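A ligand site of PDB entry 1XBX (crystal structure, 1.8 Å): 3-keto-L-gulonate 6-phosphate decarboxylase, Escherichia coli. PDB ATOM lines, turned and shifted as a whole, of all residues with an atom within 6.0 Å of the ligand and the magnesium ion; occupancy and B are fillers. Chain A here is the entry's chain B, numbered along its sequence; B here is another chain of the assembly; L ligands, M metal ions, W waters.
The side-chain carboxylate (OD2) of Asp 62 lies close to the side-chain amino group (NZ) of Lys 64 (3.8 Å). The backbone carbonyl oxygen (O) of Val 34 lies within hydrogen-bond range of the backbone NH (N) of Asp 62, 2.9 Å away. OE1 of Gln 142 is in hydrogen-bond range of NH1 of Arg 192, 3.1 Å away. O of Gly 171 lies within hydrogen-bond range of NH2 of Arg 137, at 3.4 Å. A ring nitrogen (ND1) of His 136 sits at hydrogen-bond distance from the side-chain carboxylate (OD1) of Asp 112 (2.6 Å). ND1 of His 136 lies close to OG1 of Thr 114 (3.3 Å). The backbone NH (N) of Val 139 is in hydrogen-bond range of the side-chain carboxylate (OD2) of Asp 67 of chain B. The side-chain hydroxyl of Ser 193 sits at hydrogen-bond distance from the backbone carbonyl oxygen of Leu 172, at 2.8 Å.
The magnesium ion is bound by OD2 of Asp 62 (2.0 Å), OE2 of Glu 33 (2.1 Å), O7 of the ligand (2.1 Å), water W3 (2.1 Å), water W1 (2.1 Å) and O1 of the ligand (2.2 Å).
Water W3 bridges OD1 of Asp 11 (2.7 Å) and N of Thr 36 (2.9 Å). Water W6 lies within hydrogen-bond range of O4 of the ligand, OD2 of Asp 11 and NH1 of Arg 195. Water W4 lies within hydrogen-bond range of O5 of the ligand (2.7 Å), O of Leu 172 (2.9 Å) and N of Ser 193 (3.0 Å). Water W2 lies within hydrogen-bond range of the side-chain hydroxyl (OG1) of Thr 114 (2.7 Å), the side-chain carboxylate (OD2) of Asp 67 of chain B (2.7 Å), the side-chain amino group (NZ) of Lys 64 (2.9 Å) and a ring nitrogen (NE2) of His 136 (3.3 Å).
Within 4 Å of the magnesium ion: Glu 33 and Asp 62. The nearest printed residue that does not touch the magnesium ion is Asp 11 (4.2 Å).
An oxygen (O1) of the ligand lies close to the side-chain carboxylate (OD2) of Asp 11, 2.5 Å away. The backbone NH of Gly 191 sits at hydrogen-bond distance from an oxygen (O5) of the ligand. An oxygen (O7) of the ligand sits close to the side-chain amino group (NZ) of Lys 64. O4 of the ligand is in hydrogen-bond range of N of Arg 192, at 2.9 Å. NE of Arg 192 is in salt-bridge range of O4 of the ligand. The backbone NH (N) of Gly 171 lies within hydrogen-bond range of an oxygen (O6) of the ligand (2.8 Å). An oxygen (O2) of the ligand lies within hydrogen-bond range of a ring nitrogen (NE2) of His 136, at 2.8 Å.
Residues that only touch the ligand: Ala 9 (3.3 Å), Val 139 (3.5 Å), Gly 170 (3.6 Å), Leu 172 (3.9 Å), Ile 189 (3.8 Å), Ala 190 (3.8 Å) and Asp 67 of chain B (3.8 Å). Hydrophobic or aromatic side chains within 4 Å of the ligand: Ala 9, His 136, Val 139 and Ile 189. Within 4 Å of the ligand: Ala 9, Asp 11, Glu 33, Asp 62, Lys 64, His 136, Val 139, Gly 170, Gly 171, Leu 172, Ile 189, Ala 190, Gly 191, Arg 192 and Asp 67 of chain B. The nearest printed residue that does not touch the ligand is Ala 169 (4.5 Å).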
ATOM      1  N   ALA A   9      22.949 -27.336 -17.397  1.00  0.00           N
ATOM      2  CA  ALA A   9      21.827 -26.497 -17.014  1.00  0.00           C
ATOM      3  C   ALA A   9      22.279 -25.138 -16.616  1.00  0.00           C
ATOM      4  O   ALA A   9      23.054 -25.007 -15.634  1.00  0.00           O
ATOM      5  CB  ALA A   9      21.007 -27.143 -15.853  1.00  0.00           C
ATOM      6  N   LEU A  10      21.833 -24.134 -17.371  1.00  0.00           N
ATOM      7  CA  LEU A  10      22.091 -22.753 -17.033  1.00  0.00           C
ATOM      8  C   LEU A  10      20.961 -22.228 -16.179  1.00  0.00           C
ATOM      9  O   LEU A  10      20.006 -21.647 -16.668  1.00  0.00           O
ATOM     10  CB  LEU A  10      22.339 -21.902 -18.258  1.00  0.00           C
ATOM     11  CG  LEU A  10      23.463 -22.379 -19.137  1.00  0.00           C
ATOM     12  CD1 LEU A  10      23.459 -21.562 -20.455  1.00  0.00           C
ATOM     13  CD2 LEU A  10      24.853 -22.312 -18.457  1.00  0.00           C
ATOM     14  N   ASP A  11      21.101 -22.419 -14.863  1.00  0.00           N
ATOM     15  CA  ASP A  11      20.134 -21.944 -13.889  1.00  0.00           C
ATOM     16  C   ASP A  11      20.592 -20.684 -13.207  1.00  0.00           C
ATOM     17  O   ASP A  11      20.455 -20.512 -12.041  1.00  0.00           O
ATOM     18  CB  ASP A  11      19.830 -23.015 -12.833  1.00  0.00           C
ATOM     19  CG  ASP A  11      19.007 -24.147 -13.411  1.00  0.00           C
ATOM     20  OD1 ASP A  11      17.983 -23.773 -14.053  1.00  0.00           O
ATOM     21  OD2 ASP A  11      19.302 -25.380 -13.288  1.00  0.00           O
ATOM     22  N   GLU A  33      21.210 -26.097 -21.833  1.00  0.00           N
ATOM     23  CA  GLU A  33      19.887 -25.832 -21.281  1.00  0.00           C
ATOM     24  C   GLU A  33      19.782 -24.389 -20.720  1.00  0.00           C
ATOM     25  O   GLU A  33      20.602 -23.907 -19.921  1.00  0.00           O
ATOM     26  CB  GLU A  33      19.472 -26.840 -20.226  1.00  0.00           C
ATOM     27  CG  GLU A  33      18.506 -26.303 -19.194  1.00  0.00           C
ATOM     28  CD  GLU A  33      18.157 -27.235 -18.068  1.00  0.00           C
ATOM     29  OE1 GLU A  33      18.463 -28.469 -18.126  1.00  0.00           O
ATOM     30  OE2 GLU A  33      17.595 -26.739 -17.080  1.00  0.00           O
ATOM     31  N   VAL A  34      18.757 -23.708 -21.211  1.00  0.00           N
ATOM     32  CA  VAL A  34      18.302 -22.482 -20.622  1.00  0.00           C
ATOM     33  C   VAL A  34      17.400 -22.914 -19.482  1.00  0.00           C
ATOM     34  O   VAL A  34      16.246 -23.374 -19.682  1.00  0.00           O
ATOM     35  CB  VAL A  34      17.511 -21.640 -21.612  1.00  0.00           C
ATOM     36  CG1 VAL A  34      17.158 -20.277 -20.974  1.00  0.00           C
ATOM     37  CG2 VAL A  34      18.299 -21.391 -22.855  1.00  0.00           C
ATOM     38  N   GLY A  35      17.947 -22.843 -18.259  1.00  0.00           N
ATOM     39  CA  GLY A  35      17.242 -23.332 -17.124  1.00  0.00           C
ATOM     40  C   GLY A  35      15.960 -22.570 -16.870  1.00  0.00           C
ATOM     41  O   GLY A  35      15.811 -21.413 -17.292  1.00  0.00           O
ATOM     42  N   THR A  36      15.062 -23.187 -16.118  1.00  0.00           N
ATOM     43  CA  THR A  36      13.870 -22.477 -15.711  1.00  0.00           C
ATOM     44  C   THR A  36      14.182 -21.167 -15.013  1.00  0.00           C
ATOM     45  O   THR A  36      13.503 -20.157 -15.201  1.00  0.00           O
ATOM     46  CB  THR A  36      13.042 -23.380 -14.748  1.00  0.00           C
ATOM     47  OG1 THR A  36      12.980 -24.697 -15.259  1.00  0.00           O
ATOM     48  CG2 THR A  36      11.639 -22.875 -14.684  1.00  0.00           C
ATOM     49  N   ASP A  62      14.089 -24.958 -20.688  1.00  0.00           N
ATOM     50  CA  ASP A  62      13.485 -25.731 -19.609  1.00  0.00           C
ATOM     51  C   ASP A  62      12.307 -24.984 -19.002  1.00  0.00           C
ATOM     52  O   ASP A  62      12.285 -24.616 -17.812  1.00  0.00           O
ATOM     53  CB  ASP A  62      14.552 -26.119 -18.554  1.00  0.00           C
ATOM     54  CG  ASP A  62      14.085 -27.210 -17.631  1.00  0.00           C
ATOM     55  OD1 ASP A  62      13.092 -27.912 -17.919  1.00  0.00           O
ATOM     56  OD2 ASP A  62      14.673 -27.422 -16.548  1.00  0.00           O
ATOM     57  N   LYS A  64       9.223 -25.976 -18.482  1.00  0.00           N
ATOM     58  CA  LYS A  64       8.352 -26.770 -17.633  1.00  0.00           C
ATOM     59  C   LYS A  64       6.898 -26.311 -17.773  1.00  0.00           C
ATOM     60  O   LYS A  64       6.215 -26.039 -16.804  1.00  0.00           O
ATOM     61  CB  LYS A  64       8.796 -26.813 -16.152  1.00  0.00           C
ATOM     62  CG  LYS A  64      10.175 -27.533 -15.992  1.00  0.00           C
ATOM     63  CD  LYS A  64      10.696 -27.435 -14.584  1.00  0.00           C
ATOM     64  CE  LYS A  64      12.139 -27.982 -14.528  1.00  0.00           C
ATOM     65  NZ  LYS A  64      12.829 -27.697 -13.206  1.00  0.00           N
ATOM     66  N   ASP A 112       9.049 -33.402 -18.445  1.00  0.00           N
ATOM     67  CA  ASP A 112       9.844 -33.370 -17.207  1.00  0.00           C
ATOM     68  C   ASP A 112       9.045 -34.027 -16.043  1.00  0.00           C
ATOM     69  O   ASP A 112       7.930 -33.607 -15.746  1.00  0.00           O
ATOM     70  CB  ASP A 112      10.261 -31.942 -16.857  1.00  0.00           C
ATOM     71  CG  ASP A 112      11.174 -31.906 -15.640  1.00  0.00           C
ATOM     72  OD1 ASP A 112      12.421 -31.854 -15.798  1.00  0.00           O
ATOM     73  OD2 ASP A 112      10.707 -32.026 -14.501  1.00  0.00           O
ATOM     74  N   THR A 114       9.471 -34.135 -12.705  1.00  0.00           N
ATOM     75  CA  THR A 114       9.645 -33.739 -11.309  1.00  0.00           C
ATOM     76  C   THR A 114       8.337 -33.914 -10.601  1.00  0.00           C
ATOM     77  O   THR A 114       7.298 -33.475 -11.112  1.00  0.00           O
ATOM     78  CB  THR A 114      10.090 -32.290 -11.282  1.00  0.00           C
ATOM     79  OG1 THR A 114      11.353 -32.182 -11.961  1.00  0.00           O
ATOM     80  CG2 THR A 114      10.297 -31.794  -9.868  1.00  0.00           C
ATOM     81  N   HIS A 136      13.632 -36.875 -13.116  1.00  0.00           N
ATOM     82  CA  HIS A 136      14.158 -35.695 -12.410  1.00  0.00           C
ATOM     83  C   HIS A 136      13.894 -35.801 -10.945  1.00  0.00           C
ATOM     84  O   HIS A 136      12.749 -35.755 -10.492  1.00  0.00           O
ATOM     85  CB  HIS A 136      13.459 -34.433 -13.006  1.00  0.00           C
ATOM     86  CG  HIS A 136      14.273 -33.170 -12.924  1.00  0.00           C
ATOM     87  ND1 HIS A 136      14.081 -32.100 -13.791  1.00  0.00           N
ATOM     88  CD2 HIS A 136      15.254 -32.787 -12.076  1.00  0.00           C
ATOM     89  CE1 HIS A 136      14.914 -31.132 -13.485  1.00  0.00           C
ATOM     90  NE2 HIS A 136      15.639 -31.515 -12.442  1.00  0.00           N
ATOM     91  N   ARG A 137      14.950 -35.954 -10.155  1.00  0.00           N
ATOM     92  CA  ARG A 137      14.838 -35.763  -8.716  1.00  0.00           C
ATOM     93  C   ARG A 137      14.701 -34.279  -8.388  1.00  0.00           C
ATOM     94  O   ARG A 137      15.490 -33.457  -8.829  1.00  0.00           O
ATOM     95  CB  ARG A 137      16.050 -36.349  -8.023  1.00  0.00           C
ATOM     96  CG  ARG A 137      16.066 -36.063  -6.542  1.00  0.00           C
ATOM     97  CD  ARG A 137      17.293 -36.635  -5.802  1.00  0.00           C
ATOM     98  NE  ARG A 137      18.563 -36.104  -6.292  1.00  0.00           N
ATOM     99  CZ  ARG A 137      19.757 -36.368  -5.761  1.00  0.00           C
ATOM    100  NH1 ARG A 137      19.849 -37.111  -4.656  1.00  0.00           N
ATOM    101  NH2 ARG A 137      20.872 -35.844  -6.279  1.00  0.00           N
ATOM    102  N   VAL A 139      15.081 -30.817  -6.905  1.00  0.00           N
ATOM    103  CA  VAL A 139      16.221 -30.239  -6.228  1.00  0.00           C
ATOM    104  C   VAL A 139      15.863 -29.893  -4.774  1.00  0.00           C
ATOM    105  O   VAL A 139      16.724 -29.956  -3.885  1.00  0.00           O
ATOM    106  CB  VAL A 139      16.824 -29.032  -6.993  1.00  0.00           C
ATOM    107  CG1 VAL A 139      17.279 -29.431  -8.408  1.00  0.00           C
ATOM    108  CG2 VAL A 139      15.863 -27.840  -7.099  1.00  0.00           C
ATOM    109  N   GLN A 142      16.021 -33.244  -2.973  1.00  0.00           N
ATOM    110  CA  GLN A 142      17.424 -33.481  -2.715  1.00  0.00           C
ATOM    111  C   GLN A 142      17.961 -32.680  -1.507  1.00  0.00           C
ATOM    112  O   GLN A 142      18.737 -33.229  -0.711  1.00  0.00           O
ATOM    113  CB  GLN A 142      18.252 -33.169  -3.973  1.00  0.00           C
ATOM    114  CG  GLN A 142      19.756 -33.197  -3.752  1.00  0.00           C
ATOM    115  CD  GLN A 142      20.468 -32.298  -4.762  1.00  0.00           C
ATOM    116  OE1 GLN A 142      19.816 -31.727  -5.672  1.00  0.00           O
ATOM    117  NE2 GLN A 142      21.773 -32.194  -4.643  1.00  0.00           N
ATOM    118  N   ALA A 169      18.365 -36.223 -14.248  1.00  0.00           N
ATOM    119  CA  ALA A 169      18.720 -34.937 -13.677  1.00  0.00           C
ATOM    120  C   ALA A 169      18.316 -34.845 -12.217  1.00  0.00           C
ATOM    121  O   ALA A 169      17.365 -35.529 -11.775  1.00  0.00           O
ATOM    122  CB  ALA A 169      18.024 -33.838 -14.431  1.00  0.00           C
ATOM    123  N   GLY A 170      18.934 -33.903 -11.524  1.00  0.00           N
ATOM    124  CA  GLY A 170      18.507 -33.506 -10.211  1.00  0.00           C
ATOM    125  C   GLY A 170      19.664 -33.635  -9.249  1.00  0.00           C
ATOM    126  O   GLY A 170      19.867 -34.709  -8.618  1.00  0.00           O
ATOM    127  N   GLY A 171      20.454 -32.578  -9.155  1.00  0.00           N
ATOM    128  CA  GLY A 171      21.591 -32.546  -8.247  1.00  0.00           C
ATOM    129  C   GLY A 171      22.634 -33.573  -8.572  1.00  0.00           C
ATOM    130  O   GLY A 171      23.358 -34.060  -7.693  1.00  0.00           O
ATOM    131  N   LEU A 172      22.798 -33.901  -9.842  1.00  0.00           N
ATOM    132  CA  LEU A 172      23.699 -34.948 -10.211  1.00  0.00           C
ATOM    133  C   LEU A 172      25.130 -34.622  -9.889  1.00  0.00           C
ATOM    134  O   LEU A 172      25.652 -33.563 -10.248  1.00  0.00           O
ATOM    135  CB  LEU A 172      23.582 -35.222 -11.714  1.00  0.00           C
ATOM    136  CG  LEU A 172      24.146 -36.514 -12.212  1.00  0.00           C
ATOM    137  CD1 LEU A 172      23.294 -37.688 -11.648  1.00  0.00           C
ATOM    138  CD2 LEU A 172      24.112 -36.498 -13.732  1.00  0.00           C
ATOM    139  N   ILE A 189      21.964 -34.502 -17.125  1.00  0.00           N
ATOM    140  CA  ILE A 189      22.023 -33.055 -16.925  1.00  0.00           C
ATOM    141  C   ILE A 189      22.864 -32.770 -15.694  1.00  0.00           C
ATOM    142  O   ILE A 189      22.624 -33.364 -14.645  1.00  0.00           O
ATOM    143  CB  ILE A 189      20.646 -32.422 -16.745  1.00  0.00           C
ATOM    144  CG1 ILE A 189      19.629 -32.834 -17.849  1.00  0.00           C
ATOM    145  CG2 ILE A 189      20.795 -30.910 -16.692  1.00  0.00           C
ATOM    146  CD1 ILE A 189      18.240 -32.215 -17.707  1.00  0.00           C
ATOM    147  N   ALA A 190      23.791 -31.834 -15.801  1.00  0.00           N
ATOM    148  CA  ALA A 190      24.481 -31.300 -14.630  1.00  0.00           C
ATOM    149  C   ALA A 190      24.397 -29.777 -14.651  1.00  0.00           C
ATOM    150  O   ALA A 190      24.818 -29.143 -15.631  1.00  0.00           O
ATOM    151  CB  ALA A 190      25.935 -31.710 -14.651  1.00  0.00           C
ATOM    152  N   GLY A 191      23.874 -29.189 -13.570  1.00  0.00           N
ATOM    153  CA  GLY A 191      23.834 -27.769 -13.366  1.00  0.00           C
ATOM    154  C   GLY A 191      24.940 -27.353 -12.390  1.00  0.00           C
ATOM    155  O   GLY A 191      26.042 -27.018 -12.803  1.00  0.00           O
ATOM    156  N   ARG A 192      24.643 -27.442 -11.089  1.00  0.00           N
ATOM    157  CA  ARG A 192      25.537 -26.973 -10.068  1.00  0.00           C
ATOM    158  C   ARG A 192      26.871 -27.705 -10.085  1.00  0.00           C
ATOM    159  O   ARG A 192      27.900 -27.065  -9.862  1.00  0.00           O
ATOM    160  CB  ARG A 192      24.905 -27.129  -8.663  1.00  0.00           C
ATOM    161  CG  ARG A 192      23.810 -26.116  -8.379  1.00  0.00           C
ATOM    162  CD  ARG A 192      22.859 -26.515  -7.266  1.00  0.00           C
ATOM    163  NE  ARG A 192      21.981 -27.596  -7.704  1.00  0.00           N
ATOM    164  CZ  ARG A 192      21.301 -28.406  -6.917  1.00  0.00           C
ATOM    165  NH1 ARG A 192      20.538 -29.329  -7.458  1.00  0.00           N
ATOM    166  NH2 ARG A 192      21.337 -28.261  -5.583  1.00  0.00           N
ATOM    167  N   SER A 193      26.870 -29.000 -10.351  1.00  0.00           N
ATOM    168  CA  SER A 193      28.137 -29.752 -10.346  1.00  0.00           C
ATOM    169  C   SER A 193      29.156 -29.299 -11.386  1.00  0.00           C
ATOM    170  O   SER A 193      30.367 -29.530 -11.231  1.00  0.00           O
ATOM    171  CB  SER A 193      27.852 -31.264 -10.405  1.00  0.00           C
ATOM    172  OG  SER A 193      27.106 -31.547 -11.580  1.00  0.00           O
ATOM    173  N   ARG A 195      28.617 -25.739 -12.908  1.00  0.00           N
ATOM    174  CA  ARG A 195      28.695 -24.281 -12.784  1.00  0.00           C
ATOM    175  C   ARG A 195      29.527 -23.829 -11.601  1.00  0.00           C
ATOM    176  O   ARG A 195      30.211 -22.828 -11.707  1.00  0.00           O
ATOM    177  CB  ARG A 195      27.329 -23.682 -12.650  1.00  0.00           C
ATOM    178  CG  ARG A 195      26.453 -23.790 -13.941  1.00  0.00           C
ATOM    179  CD  ARG A 195      25.309 -22.770 -13.967  1.00  0.00           C
ATOM    180  NE  ARG A 195      24.717 -22.631 -12.625  1.00  0.00           N
ATOM    181  CZ  ARG A 195      23.799 -23.473 -12.103  1.00  0.00           C
ATOM    182  NH1 ARG A 195      23.309 -24.451 -12.827  1.00  0.00           N
ATOM    183  NH2 ARG A 195      23.360 -23.318 -10.877  1.00  0.00           N
ATOM    184  N   ASP B  67       9.630 -26.664  -9.157  1.00  0.00           N
ATOM    185  CA  ASP B  67      10.803 -27.064  -8.369  1.00  0.00           C
ATOM    186  C   ASP B  67      11.673 -25.809  -8.169  1.00  0.00           C
ATOM    187  O   ASP B  67      11.472 -24.781  -8.806  1.00  0.00           O
ATOM    188  CB  ASP B  67      11.579 -28.099  -9.158  1.00  0.00           C
ATOM    189  CG  ASP B  67      12.553 -28.939  -8.295  1.00  0.00           C
ATOM    190  OD1 ASP B  67      12.506 -28.859  -7.026  1.00  0.00           O
ATOM    191  OD2 ASP B  67      13.389 -29.687  -8.869  1.00  0.00           O
ATOM    192  N   ALA B  68      12.653 -25.907  -7.274  1.00  0.00           N
ATOM    193  CA  ALA B  68      13.525 -24.798  -6.959  1.00  0.00           C
ATOM    194  C   ALA B  68      12.658 -23.702  -6.312  1.00  0.00           C
ATOM    195  O   ALA B  68      12.749 -22.512  -6.614  1.00  0.00           O
ATOM    196  CB  ALA B  68      14.293 -24.325  -8.197  1.00  0.00           C
HETATM  197  C1  LIG L   1      15.764 -28.270 -11.547  1.00  0.00           C
HETATM  198  C2  LIG L   1      16.310 -28.169 -12.862  1.00  0.00           C
HETATM  199  C3  LIG L   1      17.802 -28.134 -13.007  1.00  0.00           C
HETATM  200  O1  LIG L   1      18.168 -27.440 -14.212  1.00  0.00           O
HETATM  201  C4  LIG L   1      18.347 -29.561 -13.017  1.00  0.00           C
HETATM  202  O2  LIG L   1      18.068 -30.256 -11.774  1.00  0.00           O
HETATM  203  C5  LIG L   1      19.844 -29.549 -13.305  1.00  0.00           C
HETATM  204  O3  LIG L   1      20.548 -28.721 -12.374  1.00  0.00           O
HETATM  205  P1  LIG L   1      21.334 -29.369 -11.063  1.00  0.00           P
HETATM  206  O4  LIG L   1      21.945 -28.121 -10.459  1.00  0.00           O
HETATM  207  O5  LIG L   1      22.334 -30.403 -11.578  1.00  0.00           O
HETATM  208  O6  LIG L   1      20.234 -29.983 -10.210  1.00  0.00           O
HETATM  209  O7  LIG L   1      15.520 -28.146 -13.822  1.00  0.00           O
HETATM  210 MG    MG M   1      16.435 -27.440 -15.529  1.00  0.00          MG
HETATM  211  O   HOH W   1      16.801 -29.401 -16.223  1.00  0.00           O
HETATM  212  O   HOH W   2      12.836 -30.023 -11.525  1.00  0.00           O
HETATM  213  O   HOH W   3      16.062 -25.517 -14.772  1.00  0.00           O
HETATM  214  O   HOH W   4      24.561 -30.886 -10.162  1.00  0.00           O
HETATM  215  O   HOH W   5      16.651 -25.715 -10.294  1.00  0.00           O
HETATM  216  O   HOH W   6      21.255 -25.776 -11.450  1.00  0.00           O
HETATM  217  O   HOH W   7      21.424 -32.787 -12.278  1.00  0.00           O
